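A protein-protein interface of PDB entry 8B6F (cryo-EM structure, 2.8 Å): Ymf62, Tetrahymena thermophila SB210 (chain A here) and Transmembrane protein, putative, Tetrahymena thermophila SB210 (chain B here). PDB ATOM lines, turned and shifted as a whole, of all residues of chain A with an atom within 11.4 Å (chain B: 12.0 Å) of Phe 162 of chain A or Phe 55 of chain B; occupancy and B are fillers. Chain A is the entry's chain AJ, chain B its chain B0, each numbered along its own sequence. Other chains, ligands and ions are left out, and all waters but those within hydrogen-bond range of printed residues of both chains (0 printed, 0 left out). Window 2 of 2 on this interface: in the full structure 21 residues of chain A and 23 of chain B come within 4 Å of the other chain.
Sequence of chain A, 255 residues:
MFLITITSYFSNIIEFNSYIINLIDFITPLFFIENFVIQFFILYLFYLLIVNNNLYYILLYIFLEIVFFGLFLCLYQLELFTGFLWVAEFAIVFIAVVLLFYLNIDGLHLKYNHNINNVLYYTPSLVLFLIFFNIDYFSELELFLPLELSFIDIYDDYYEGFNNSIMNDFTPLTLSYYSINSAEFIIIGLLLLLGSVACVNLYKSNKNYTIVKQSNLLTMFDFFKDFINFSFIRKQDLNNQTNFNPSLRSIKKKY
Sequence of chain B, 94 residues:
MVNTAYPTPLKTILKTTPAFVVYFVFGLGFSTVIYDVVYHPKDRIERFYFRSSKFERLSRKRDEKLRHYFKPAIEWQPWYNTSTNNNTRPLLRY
NZ of Lys 54 of chain B is in salt-bridge range of OE1 of Glu 160 of chain A (3.4 Å). OD1 of Asp 156 of chain A is in salt-bridge range of NZ of Lys 65 of chain B (3.1 Å). The side-chain sulfur of Met 167 of chain A sits close to the backbone carbonyl oxygen of Ser 52 of chain B.
The backbone carbonyl oxygen of Phe 50 of chain B sits at hydrogen-bond distance from the guanidinium group of Arg 57 of chain B, at 2.9 Å. OG of Ser 52 of chain B lies within hydrogen-bond range of OE1 of Glu 56 of chain B (2.7 Å). The side-chain carboxylate (OD1) of Asp 157 of chain A sits at hydrogen-bond distance from the backbone NH (N) of Glu 160 of chain A. The backbone carbonyl oxygen of Phe 55 of chain B lies within hydrogen-bond range of the side-chain hydroxyl of Ser 59 of chain B, at 3.3 Å. NH2 of Arg 62 of chain B lies within salt-bridge range of OD1 of Asp 63 of chain B (3.5 Å). ND2 of Asn 164 of chain A lies within hydrogen-bond range of OE2 of Glu 160 of chain A (3.3 Å).
Asp 157 of chain A touches Leu 58 of chain B (O to CD2, 3.8 Å). Tyr 158 of chain A touches Phe 55 of chain B. Tyr 158 of chain A touches Leu 58 of chain B (CE2 to CB, 3.9 Å). Arg 62 of chain B touches Tyr 158 of chain A. Gly 161 of chain A touches Lys 54 of chain B. O of Gly 161 of chain A touches N of Phe 55 of chain B (3.7 Å). CB of Phe 162 of chain A touches CD2 of Phe 55 of chain B (3.98 Å). O of Phe 50 of chain B touches CE of Met 167 of chain A (3.5 Å). Met 167 of chain A touches Arg 51 of chain B (CE to NH1, 3.2 Å). Met 167 of chain A touches Arg 57 of chain B (SD to NH2, 3.8 Å).
Of chain B, only Phe 55 (3.98 Å) comes within 4 Å of Phe 162 of chain A. No residue of chain B comes within 4 Å of Tyr 159 of chain A. Of chain B, only Lys 54 comes within 4 Å of Glu 160 of chain A. Gly 161 of chain A touches just these residues of chain B: Lys 54 (3.4 Å) and Phe 55 (3.7 Å). No residue of chain B comes within 4 Å of Asn 163 of chain A. No residue of chain B comes within 4 Å of Asn 164 of chain A. No residue of chain A comes within 4 Å of Ser 53 of chain B. Lys 54 of chain B touches two residues of chain A. No residue of chain A comes within 4 Å of Glu 56 of chain B. Leu 58 of chain B touches just these residues of chain A: Asp 157 (3.8 Å) and Tyr 158 (3.9 Å). Ser 59 of chain B touches none of the printed residues of chain A. Of the printed residues of chain A, Arg 51 of chain B touches Met 167 (3.2 Å). Of the printed residues of chain A, Arg 57 of chain B touches Met 167 (3.8 Å). Tyr 49 of chain B touches none of the printed residues of chain A. The nearest printed residue of chain A that does not touch Arg 62 of chain B is Asp 156 of chain A (4.7 Å).
Of the 19 printed residues of chain B, 9 touch a printed residue of chain A.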
ATOM      1  N   ASP A 156     -23.913  -8.794 -25.284  1.00  0.00           N
ATOM      2  CA  ASP A 156     -22.930  -7.894 -25.870  1.00  0.00           C
ATOM      3  C   ASP A 156     -21.751  -8.703 -26.385  1.00  0.00           C
ATOM      4  O   ASP A 156     -21.299  -9.647 -25.730  1.00  0.00           O
ATOM      5  CB  ASP A 156     -22.440  -6.856 -24.854  1.00  0.00           C
ATOM      6  CG  ASP A 156     -23.556  -5.963 -24.350  1.00  0.00           C
ATOM      7  OD1 ASP A 156     -24.505  -5.708 -25.119  1.00  0.00           O
ATOM      8  OD2 ASP A 156     -23.481  -5.514 -23.188  1.00  0.00           O
ATOM      9  N   ASP A 157     -21.252  -8.326 -27.556  1.00  0.00           N
ATOM     10  CA  ASP A 157     -20.125  -8.993 -28.200  1.00  0.00           C
ATOM     11  C   ASP A 157     -18.924  -8.057 -28.128  1.00  0.00           C
ATOM     12  O   ASP A 157     -18.760  -7.176 -28.976  1.00  0.00           O
ATOM     13  CB  ASP A 157     -20.467  -9.359 -29.641  1.00  0.00           C
ATOM     14  CG  ASP A 157     -19.409 -10.224 -30.289  1.00  0.00           C
ATOM     15  OD1 ASP A 157     -18.413 -10.555 -29.612  1.00  0.00           O
ATOM     16  OD2 ASP A 157     -19.570 -10.574 -31.475  1.00  0.00           O
ATOM     17  N   TYR A 158     -18.088  -8.246 -27.104  1.00  0.00           N
ATOM     18  CA  TYR A 158     -16.978  -7.326 -26.881  1.00  0.00           C
ATOM     19  C   TYR A 158     -15.857  -7.532 -27.890  1.00  0.00           C
ATOM     20  O   TYR A 158     -15.178  -6.568 -28.258  1.00  0.00           O
ATOM     21  CB  TYR A 158     -16.452  -7.478 -25.455  1.00  0.00           C
ATOM     22  CG  TYR A 158     -17.463  -7.060 -24.418  1.00  0.00           C
ATOM     23  CD1 TYR A 158     -18.398  -7.960 -23.931  1.00  0.00           C
ATOM     24  CD2 TYR A 158     -17.491  -5.758 -23.937  1.00  0.00           C
ATOM     25  CE1 TYR A 158     -19.328  -7.580 -22.990  1.00  0.00           C
ATOM     26  CE2 TYR A 158     -18.417  -5.367 -22.995  1.00  0.00           C
ATOM     27  CZ  TYR A 158     -19.334  -6.282 -22.526  1.00  0.00           C
ATOM     28  OH  TYR A 158     -20.260  -5.898 -21.589  1.00  0.00           O
ATOM     29  N   TYR A 159     -15.643  -8.767 -28.346  1.00  0.00           N
ATOM     30  CA  TYR A 159     -14.630  -9.000 -29.370  1.00  0.00           C
ATOM     31  C   TYR A 159     -14.978  -8.259 -30.653  1.00  0.00           C
ATOM     32  O   TYR A 159     -14.138  -7.559 -31.229  1.00  0.00           O
ATOM     33  CB  TYR A 159     -14.468 -10.496 -29.626  1.00  0.00           C
ATOM     34  CG  TYR A 159     -13.552 -11.169 -28.633  1.00  0.00           C
ATOM     35  CD1 TYR A 159     -14.038 -11.665 -27.431  1.00  0.00           C
ATOM     36  CD2 TYR A 159     -12.194 -11.292 -28.892  1.00  0.00           C
ATOM     37  CE1 TYR A 159     -13.196 -12.276 -26.521  1.00  0.00           C
ATOM     38  CE2 TYR A 159     -11.346 -11.899 -27.992  1.00  0.00           C
ATOM     39  CZ  TYR A 159     -11.852 -12.389 -26.808  1.00  0.00           C
ATOM     40  OH  TYR A 159     -11.006 -12.994 -25.912  1.00  0.00           O
ATOM     41  N   GLU A 160     -16.214  -8.411 -31.124  1.00  0.00           N
ATOM     42  CA  GLU A 160     -16.658  -7.649 -32.284  1.00  0.00           C
ATOM     43  C   GLU A 160     -16.652  -6.156 -31.994  1.00  0.00           C
ATOM     44  O   GLU A 160     -16.395  -5.349 -32.893  1.00  0.00           O
ATOM     45  CB  GLU A 160     -18.052  -8.108 -32.713  1.00  0.00           C
ATOM     46  CG  GLU A 160     -18.491  -7.594 -34.080  1.00  0.00           C
ATOM     47  CD  GLU A 160     -19.005  -6.166 -34.046  1.00  0.00           C
ATOM     48  OE1 GLU A 160     -19.298  -5.661 -32.943  1.00  0.00           O
ATOM     49  OE2 GLU A 160     -19.121  -5.551 -35.127  1.00  0.00           O
ATOM     50  N   GLY A 161     -16.936  -5.770 -30.750  1.00  0.00           N
ATOM     51  CA  GLY A 161     -16.926  -4.357 -30.407  1.00  0.00           C
ATOM     52  C   GLY A 161     -15.561  -3.719 -30.581  1.00  0.00           C
ATOM     53  O   GLY A 161     -15.439  -2.642 -31.167  1.00  0.00           O
ATOM     54  N   PHE A 162     -14.516  -4.374 -30.080  1.00  0.00           N
ATOM     55  CA  PHE A 162     -13.175  -3.821 -30.219  1.00  0.00           C
ATOM     56  C   PHE A 162     -12.605  -4.017 -31.616  1.00  0.00           C
ATOM     57  O   PHE A 162     -11.671  -3.302 -31.992  1.00  0.00           O
ATOM     58  CB  PHE A 162     -12.240  -4.428 -29.163  1.00  0.00           C
ATOM     59  CG  PHE A 162     -11.426  -5.592 -29.653  1.00  0.00           C
ATOM     60  CD1 PHE A 162     -10.237  -5.397 -30.336  1.00  0.00           C
ATOM     61  CD2 PHE A 162     -11.824  -6.884 -29.375  1.00  0.00           C
ATOM     62  CE1 PHE A 162      -9.486  -6.473 -30.768  1.00  0.00           C
ATOM     63  CE2 PHE A 162     -11.081  -7.966 -29.801  1.00  0.00           C
ATOM     64  CZ  PHE A 162      -9.909  -7.760 -30.499  1.00  0.00           C
ATOM     65  N   ASN A 163     -13.142  -4.957 -32.392  1.00  0.00           N
ATOM     66  CA  ASN A 163     -12.771  -5.076 -33.795  1.00  0.00           C
ATOM     67  C   ASN A 163     -13.534  -4.109 -34.689  1.00  0.00           C
ATOM     68  O   ASN A 163     -13.172  -3.960 -35.861  1.00  0.00           O
ATOM     69  CB  ASN A 163     -13.012  -6.506 -34.289  1.00  0.00           C
ATOM     70  CG  ASN A 163     -11.996  -7.488 -33.747  1.00  0.00           C
ATOM     71  OD1 ASN A 163     -12.355  -8.483 -33.116  1.00  0.00           O
ATOM     72  ND2 ASN A 163     -10.720  -7.217 -33.990  1.00  0.00           N
ATOM     73  N   ASN A 164     -14.571  -3.455 -34.174  1.00  0.00           N
ATOM     74  CA  ASN A 164     -15.379  -2.537 -34.963  1.00  0.00           C
ATOM     75  C   ASN A 164     -14.810  -1.129 -34.851  1.00  0.00           C
ATOM     76  O   ASN A 164     -14.608  -0.620 -33.744  1.00  0.00           O
ATOM     77  CB  ASN A 164     -16.831  -2.565 -34.484  1.00  0.00           C
ATOM     78  CG  ASN A 164     -17.771  -1.847 -35.427  1.00  0.00           C
ATOM     79  OD1 ASN A 164     -17.370  -0.933 -36.145  1.00  0.00           O
ATOM     80  ND2 ASN A 164     -19.033  -2.257 -35.429  1.00  0.00           N
ATOM     81  N   SER A 165     -14.558  -0.502 -35.998  1.00  0.00           N
ATOM     82  CA  SER A 165     -14.012   0.846 -36.052  1.00  0.00           C
ATOM     83  C   SER A 165     -15.003   1.871 -36.585  1.00  0.00           C
ATOM     84  O   SER A 165     -14.636   3.039 -36.748  1.00  0.00           O
ATOM     85  CB  SER A 165     -12.741   0.863 -36.909  1.00  0.00           C
ATOM     86  OG  SER A 165     -13.018   0.451 -38.237  1.00  0.00           O
ATOM     87  N   ILE A 166     -16.245   1.472 -36.858  1.00  0.00           N
ATOM     88  CA  ILE A 166     -17.223   2.394 -37.417  1.00  0.00           C
ATOM     89  C   ILE A 166     -17.604   3.441 -36.378  1.00  0.00           C
ATOM     90  O   ILE A 166     -17.651   3.170 -35.171  1.00  0.00           O
ATOM     91  CB  ILE A 166     -18.459   1.619 -37.911  1.00  0.00           C
ATOM     92  CG1 ILE A 166     -18.060   0.653 -39.030  1.00  0.00           C
ATOM     93  CG2 ILE A 166     -19.541   2.575 -38.399  1.00  0.00           C
ATOM     94  CD1 ILE A 166     -19.106  -0.393 -39.332  1.00  0.00           C
ATOM     95  N   MET A 167     -17.889   4.656 -36.855  1.00  0.00           N
ATOM     96  CA  MET A 167     -18.268   5.761 -35.989  1.00  0.00           C
ATOM     97  C   MET A 167     -19.510   6.509 -36.455  1.00  0.00           C
ATOM     98  O   MET A 167     -19.949   7.431 -35.761  1.00  0.00           O
ATOM     99  CB  MET A 167     -17.109   6.759 -35.860  1.00  0.00           C
ATOM    100  CG  MET A 167     -16.072   6.355 -34.834  1.00  0.00           C
ATOM    101  SD  MET A 167     -16.704   6.429 -33.145  1.00  0.00           S
ATOM    102  CE  MET A 167     -16.823   8.198 -32.902  1.00  0.00           C
ATOM    103  N   ARG B  47     -18.909  12.673 -21.763  1.00  0.00           N
ATOM    104  CA  ARG B  47     -18.795  12.714 -23.212  1.00  0.00           C
ATOM    105  C   ARG B  47     -20.046  12.132 -23.854  1.00  0.00           C
ATOM    106  O   ARG B  47     -20.681  11.219 -23.319  1.00  0.00           O
ATOM    107  CB  ARG B  47     -17.555  11.946 -23.674  1.00  0.00           C
ATOM    108  CG  ARG B  47     -16.265  12.434 -23.036  1.00  0.00           C
ATOM    109  CD  ARG B  47     -15.033  11.878 -23.734  1.00  0.00           C
ATOM    110  NE  ARG B  47     -14.934  10.427 -23.628  1.00  0.00           N
ATOM    111  CZ  ARG B  47     -15.390   9.568 -24.530  1.00  0.00           C
ATOM    112  NH1 ARG B  47     -16.003   9.977 -25.629  1.00  0.00           N
ATOM    113  NH2 ARG B  47     -15.229   8.265 -24.324  1.00  0.00           N
ATOM    114  N   PHE B  48     -20.405  12.673 -25.015  1.00  0.00           N
ATOM    115  CA  PHE B  48     -21.569  12.171 -25.728  1.00  0.00           C
ATOM    116  C   PHE B  48     -21.393  10.692 -26.039  1.00  0.00           C
ATOM    117  O   PHE B  48     -20.286  10.208 -26.283  1.00  0.00           O
ATOM    118  CB  PHE B  48     -21.791  12.949 -27.027  1.00  0.00           C
ATOM    119  CG  PHE B  48     -22.279  14.361 -26.830  1.00  0.00           C
ATOM    120  CD1 PHE B  48     -22.916  14.744 -25.661  1.00  0.00           C
ATOM    121  CD2 PHE B  48     -22.108  15.301 -27.831  1.00  0.00           C
ATOM    122  CE1 PHE B  48     -23.367  16.036 -25.496  1.00  0.00           C
ATOM    123  CE2 PHE B  48     -22.556  16.594 -27.670  1.00  0.00           C
ATOM    124  CZ  PHE B  48     -23.186  16.962 -26.501  1.00  0.00           C
ATOM    125  N   TYR B  49     -22.512   9.970 -26.020  1.00  0.00           N
ATOM    126  CA  TYR B  49     -22.464   8.532 -26.252  1.00  0.00           C
ATOM    127  C   TYR B  49     -21.905   8.213 -27.631  1.00  0.00           C
ATOM    128  O   TYR B  49     -21.075   7.309 -27.779  1.00  0.00           O
ATOM    129  CB  TYR B  49     -23.862   7.942 -26.087  1.00  0.00           C
ATOM    130  CG  TYR B  49     -23.930   6.462 -26.342  1.00  0.00           C
ATOM    131  CD1 TYR B  49     -23.500   5.558 -25.386  1.00  0.00           C
ATOM    132  CD2 TYR B  49     -24.440   5.968 -27.531  1.00  0.00           C
ATOM    133  CE1 TYR B  49     -23.564   4.207 -25.607  1.00  0.00           C
ATOM    134  CE2 TYR B  49     -24.509   4.616 -27.763  1.00  0.00           C
ATOM    135  CZ  TYR B  49     -24.071   3.742 -26.796  1.00  0.00           C
ATOM    136  OH  TYR B  49     -24.138   2.395 -27.028  1.00  0.00           O
ATOM    137  N   PHE B  50     -22.337   8.951 -28.655  1.00  0.00           N
ATOM    138  CA  PHE B  50     -21.884   8.690 -30.014  1.00  0.00           C
ATOM    139  C   PHE B  50     -20.444   9.121 -30.253  1.00  0.00           C
ATOM    140  O   PHE B  50     -19.862   8.730 -31.270  1.00  0.00           O
ATOM    141  CB  PHE B  50     -22.804   9.386 -31.019  1.00  0.00           C
ATOM    142  CG  PHE B  50     -22.931  10.864 -30.804  1.00  0.00           C
ATOM    143  CD1 PHE B  50     -22.039  11.743 -31.396  1.00  0.00           C
ATOM    144  CD2 PHE B  50     -23.950  11.377 -30.018  1.00  0.00           C
ATOM    145  CE1 PHE B  50     -22.157  13.103 -31.202  1.00  0.00           C
ATOM    146  CE2 PHE B  50     -24.074  12.735 -29.820  1.00  0.00           C
ATOM    147  CZ  PHE B  50     -23.177  13.600 -30.413  1.00  0.00           C
ATOM    148  N   ARG B  51     -19.859   9.908 -29.356  1.00  0.00           N
ATOM    149  CA  ARG B  51     -18.446  10.269 -29.442  1.00  0.00           C
ATOM    150  C   ARG B  51     -17.581   9.245 -28.718  1.00  0.00           C
ATOM    151  O   ARG B  51     -16.767   9.587 -27.863  1.00  0.00           O
ATOM    152  CB  ARG B  51     -18.224  11.662 -28.866  1.00  0.00           C
ATOM    153  CG  ARG B  51     -18.971  12.770 -29.581  1.00  0.00           C
ATOM    154  CD  ARG B  51     -18.471  12.986 -31.000  1.00  0.00           C
ATOM    155  NE  ARG B  51     -17.031  13.219 -31.055  1.00  0.00           N
ATOM    156  CZ  ARG B  51     -16.141  12.390 -31.588  1.00  0.00           C
ATOM    157  NH1 ARG B  51     -16.502  11.248 -32.153  1.00  0.00           N
ATOM    158  NH2 ARG B  51     -14.855  12.721 -31.566  1.00  0.00           N
ATOM    159  N   SER B  52     -17.756   7.971 -29.055  1.00  0.00           N
ATOM    160  CA  SER B  52     -17.064   6.909 -28.341  1.00  0.00           C
ATOM    161  C   SER B  52     -17.001   5.677 -29.231  1.00  0.00           C
ATOM    162  O   SER B  52     -17.828   5.493 -30.127  1.00  0.00           O
ATOM    163  CB  SER B  52     -17.768   6.591 -27.017  1.00  0.00           C
ATOM    164  OG  SER B  52     -16.955   5.795 -26.178  1.00  0.00           O
ATOM    165  N   SER B  53     -16.007   4.834 -28.967  1.00  0.00           N
ATOM    166  CA  SER B  53     -15.843   3.603 -29.722  1.00  0.00           C
ATOM    167  C   SER B  53     -16.938   2.603 -29.357  1.00  0.00           C
ATOM    168  O   SER B  53     -17.648   2.749 -28.360  1.00  0.00           O
ATOM    169  CB  SER B  53     -14.470   2.989 -29.454  1.00  0.00           C
ATOM    170  OG  SER B  53     -13.441   3.937 -29.653  1.00  0.00           O
ATOM    171  N   LYS B  54     -17.060   1.561 -30.181  1.00  0.00           N
ATOM    172  CA  LYS B  54     -18.058   0.530 -29.916  1.00  0.00           C
ATOM    173  C   LYS B  54     -17.790  -0.149 -28.580  1.00  0.00           C
ATOM    174  O   LYS B  54     -18.703  -0.336 -27.770  1.00  0.00           O
ATOM    175  CB  LYS B  54     -18.065  -0.491 -31.055  1.00  0.00           C
ATOM    176  CG  LYS B  54     -19.127  -1.573 -30.928  1.00  0.00           C
ATOM    177  CD  LYS B  54     -20.529  -1.009 -31.069  1.00  0.00           C
ATOM    178  CE  LYS B  54     -21.576  -2.113 -31.039  1.00  0.00           C
ATOM    179  NZ  LYS B  54     -21.410  -3.079 -32.160  1.00  0.00           N
ATOM    180  N   PHE B  55     -16.534  -0.521 -28.331  1.00  0.00           N
ATOM    181  CA  PHE B  55     -16.195  -1.166 -27.068  1.00  0.00           C
ATOM    182  C   PHE B  55     -16.445  -0.235 -25.889  1.00  0.00           C
ATOM    183  O   PHE B  55     -16.950  -0.661 -24.846  1.00  0.00           O
ATOM    184  CB  PHE B  55     -14.739  -1.627 -27.089  1.00  0.00           C
ATOM    185  CG  PHE B  55     -14.340  -2.423 -25.883  1.00  0.00           C
ATOM    186  CD1 PHE B  55     -13.888  -1.790 -24.738  1.00  0.00           C
ATOM    187  CD2 PHE B  55     -14.416  -3.804 -25.894  1.00  0.00           C
ATOM    188  CE1 PHE B  55     -13.521  -2.519 -23.627  1.00  0.00           C
ATOM    189  CE2 PHE B  55     -14.050  -4.539 -24.785  1.00  0.00           C
ATOM    190  CZ  PHE B  55     -13.602  -3.896 -23.650  1.00  0.00           C
ATOM    191  N   GLU B  56     -16.097   1.045 -26.038  1.00  0.00           N
ATOM    192  CA  GLU B  56     -16.338   2.004 -24.964  1.00  0.00           C
ATOM    193  C   GLU B  56     -17.828   2.152 -24.687  1.00  0.00           C
ATOM    194  O   GLU B  56     -18.247   2.214 -23.526  1.00  0.00           O
ATOM    195  CB  GLU B  56     -15.722   3.357 -25.315  1.00  0.00           C
ATOM    196  CG  GLU B  56     -14.202   3.360 -25.313  1.00  0.00           C
ATOM    197  CD  GLU B  56     -13.623   4.737 -25.568  1.00  0.00           C
ATOM    198  OE1 GLU B  56     -14.357   5.732 -25.392  1.00  0.00           O
ATOM    199  OE2 GLU B  56     -12.438   4.825 -25.949  1.00  0.00           O
ATOM    200  N   ARG B  57     -18.643   2.203 -25.740  1.00  0.00           N
ATOM    201  CA  ARG B  57     -20.087   2.285 -25.551  1.00  0.00           C
ATOM    202  C   ARG B  57     -20.604   1.069 -24.796  1.00  0.00           C
ATOM    203  O   ARG B  57     -21.408   1.196 -23.865  1.00  0.00           O
ATOM    204  CB  ARG B  57     -20.782   2.399 -26.906  1.00  0.00           C
ATOM    205  CG  ARG B  57     -20.488   3.681 -27.661  1.00  0.00           C
ATOM    206  CD  ARG B  57     -20.832   3.525 -29.131  1.00  0.00           C
ATOM    207  NE  ARG B  57     -20.491   4.708 -29.908  1.00  0.00           N
ATOM    208  CZ  ARG B  57     -20.591   4.790 -31.227  1.00  0.00           C
ATOM    209  NH1 ARG B  57     -21.011   3.768 -31.953  1.00  0.00           N
ATOM    210  NH2 ARG B  57     -20.259   5.926 -31.835  1.00  0.00           N
ATOM    211  N   LEU B  58     -20.153  -0.123 -25.186  1.00  0.00           N
ATOM    212  CA  LEU B  58     -20.592  -1.336 -24.508  1.00  0.00           C
ATOM    213  C   LEU B  58     -20.199  -1.317 -23.035  1.00  0.00           C
ATOM    214  O   LEU B  58     -21.007  -1.659 -22.165  1.00  0.00           O
ATOM    215  CB  LEU B  58     -20.005  -2.559 -25.210  1.00  0.00           C
ATOM    216  CG  LEU B  58     -20.852  -3.169 -26.330  1.00  0.00           C
ATOM    217  CD1 LEU B  58     -21.479  -2.099 -27.215  1.00  0.00           C
ATOM    218  CD2 LEU B  58     -20.011  -4.115 -27.167  1.00  0.00           C
ATOM    219  N   SER B  59     -18.960  -0.921 -22.738  1.00  0.00           N
ATOM    220  CA  SER B  59     -18.509  -0.884 -21.351  1.00  0.00           C
ATOM    221  C   SER B  59     -19.294   0.141 -20.545  1.00  0.00           C
ATOM    222  O   SER B  59     -19.616  -0.094 -19.375  1.00  0.00           O
ATOM    223  CB  SER B  59     -17.013  -0.582 -21.289  1.00  0.00           C
ATOM    224  OG  SER B  59     -16.729   0.701 -21.819  1.00  0.00           O
ATOM    225  N   ARG B  60     -19.597   1.292 -21.147  1.00  0.00           N
ATOM    226  CA  ARG B  60     -20.352   2.320 -20.436  1.00  0.00           C
ATOM    227  C   ARG B  60     -21.766   1.855 -20.110  1.00  0.00           C
ATOM    228  O   ARG B  60     -22.261   2.092 -19.003  1.00  0.00           O
ATOM    229  CB  ARG B  60     -20.392   3.600 -21.271  1.00  0.00           C
ATOM    230  CG  ARG B  60     -19.045   4.288 -21.409  1.00  0.00           C
ATOM    231  CD  ARG B  60     -19.053   5.327 -22.521  1.00  0.00           C
ATOM    232  NE  ARG B  60     -19.845   6.503 -22.178  1.00  0.00           N
ATOM    233  CZ  ARG B  60     -20.007   7.553 -22.970  1.00  0.00           C
ATOM    234  NH1 ARG B  60     -19.452   7.607 -24.170  1.00  0.00           N
ATOM    235  NH2 ARG B  60     -20.747   8.574 -22.549  1.00  0.00           N
ATOM    236  N   LYS B  61     -22.433   1.196 -21.055  1.00  0.00           N
ATOM    237  CA  LYS B  61     -23.834   0.831 -20.891  1.00  0.00           C
ATOM    238  C   LYS B  61     -24.038  -0.545 -20.272  1.00  0.00           C
ATOM    239  O   LYS B  61     -25.183  -0.913 -19.997  1.00  0.00           O
ATOM    240  CB  LYS B  61     -24.551   0.885 -22.243  1.00  0.00           C
ATOM    241  CG  LYS B  61     -24.519   2.256 -22.901  1.00  0.00           C
ATOM    242  CD  LYS B  61     -25.260   3.295 -22.070  1.00  0.00           C
ATOM    243  CE  LYS B  61     -25.127   4.680 -22.677  1.00  0.00           C
ATOM    244  NZ  LYS B  61     -25.868   5.702 -21.889  1.00  0.00           N
ATOM    245  N   ARG B  62     -22.970  -1.313 -20.047  1.00  0.00           N
ATOM    246  CA  ARG B  62     -23.126  -2.633 -19.445  1.00  0.00           C
ATOM    247  C   ARG B  62     -23.784  -2.539 -18.074  1.00  0.00           C
ATOM    248  O   ARG B  62     -24.722  -3.282 -17.769  1.00  0.00           O
ATOM    249  CB  ARG B  62     -21.765  -3.322 -19.343  1.00  0.00           C
ATOM    250  CG  ARG B  62     -21.829  -4.754 -18.836  1.00  0.00           C
ATOM    251  CD  ARG B  62     -20.436  -5.327 -18.653  1.00  0.00           C
ATOM    252  NE  ARG B  62     -19.802  -4.864 -17.423  1.00  0.00           N
ATOM    253  CZ  ARG B  62     -19.787  -5.535 -16.279  1.00  0.00           C
ATOM    254  NH1 ARG B  62     -20.362  -6.721 -16.162  1.00  0.00           N
ATOM    255  NH2 ARG B  62     -19.176  -5.005 -15.225  1.00  0.00           N
ATOM    256  N   ASP B  63     -23.311  -1.617 -17.234  1.00  0.00           N
ATOM    257  CA  ASP B  63     -23.843  -1.512 -15.879  1.00  0.00           C
ATOM    258  C   ASP B  63     -25.308  -1.102 -15.889  1.00  0.00           C
ATOM    259  O   ASP B  63     -26.112  -1.628 -15.111  1.00  0.00           O
ATOM    260  CB  ASP B  63     -23.013  -0.521 -15.068  1.00  0.00           C
ATOM    261  CG  ASP B  63     -21.621  -1.036 -14.775  1.00  0.00           C
ATOM    262  OD1 ASP B  63     -21.314  -2.176 -15.179  1.00  0.00           O
ATOM    263  OD2 ASP B  63     -20.836  -0.303 -14.139  1.00  0.00           O
ATOM    264  N   GLU B  64     -25.677  -0.154 -16.752  1.00  0.00           N
ATOM    265  CA  GLU B  64     -27.075   0.252 -16.840  1.00  0.00           C
ATOM    266  C   GLU B  64     -27.951  -0.906 -17.294  1.00  0.00           C
ATOM    267  O   GLU B  64     -29.042  -1.118 -16.755  1.00  0.00           O
ATOM    268  CB  GLU B  64     -27.218   1.441 -17.790  1.00  0.00           C
ATOM    269  CG  GLU B  64     -26.490   2.688 -17.322  1.00  0.00           C
ATOM    270  CD  GLU B  64     -26.728   3.878 -18.231  1.00  0.00           C
ATOM    271  OE1 GLU B  64     -27.428   3.717 -19.251  1.00  0.00           O
ATOM    272  OE2 GLU B  64     -26.215   4.975 -17.924  1.00  0.00           O
ATOM    273  N   LYS B  65     -27.496  -1.662 -18.295  1.00  0.00           N
ATOM    274  CA  LYS B  65     -28.260  -2.822 -18.739  1.00  0.00           C
ATOM    275  C   LYS B  65     -28.428  -3.826 -17.609  1.00  0.00           C
ATOM    276  O   LYS B  65     -29.524  -4.358 -17.398  1.00  0.00           O
ATOM    277  CB  LYS B  65     -27.571  -3.477 -19.937  1.00  0.00           C
ATOM    278  CG  LYS B  65     -27.582  -2.631 -21.199  1.00  0.00           C
ATOM    279  CD  LYS B  65     -26.742  -3.261 -22.296  1.00  0.00           C
ATOM    280  CE  LYS B  65     -26.723  -2.390 -23.541  1.00  0.00           C
ATOM    281  NZ  LYS B  65     -25.877  -2.974 -24.620  1.00  0.00           N
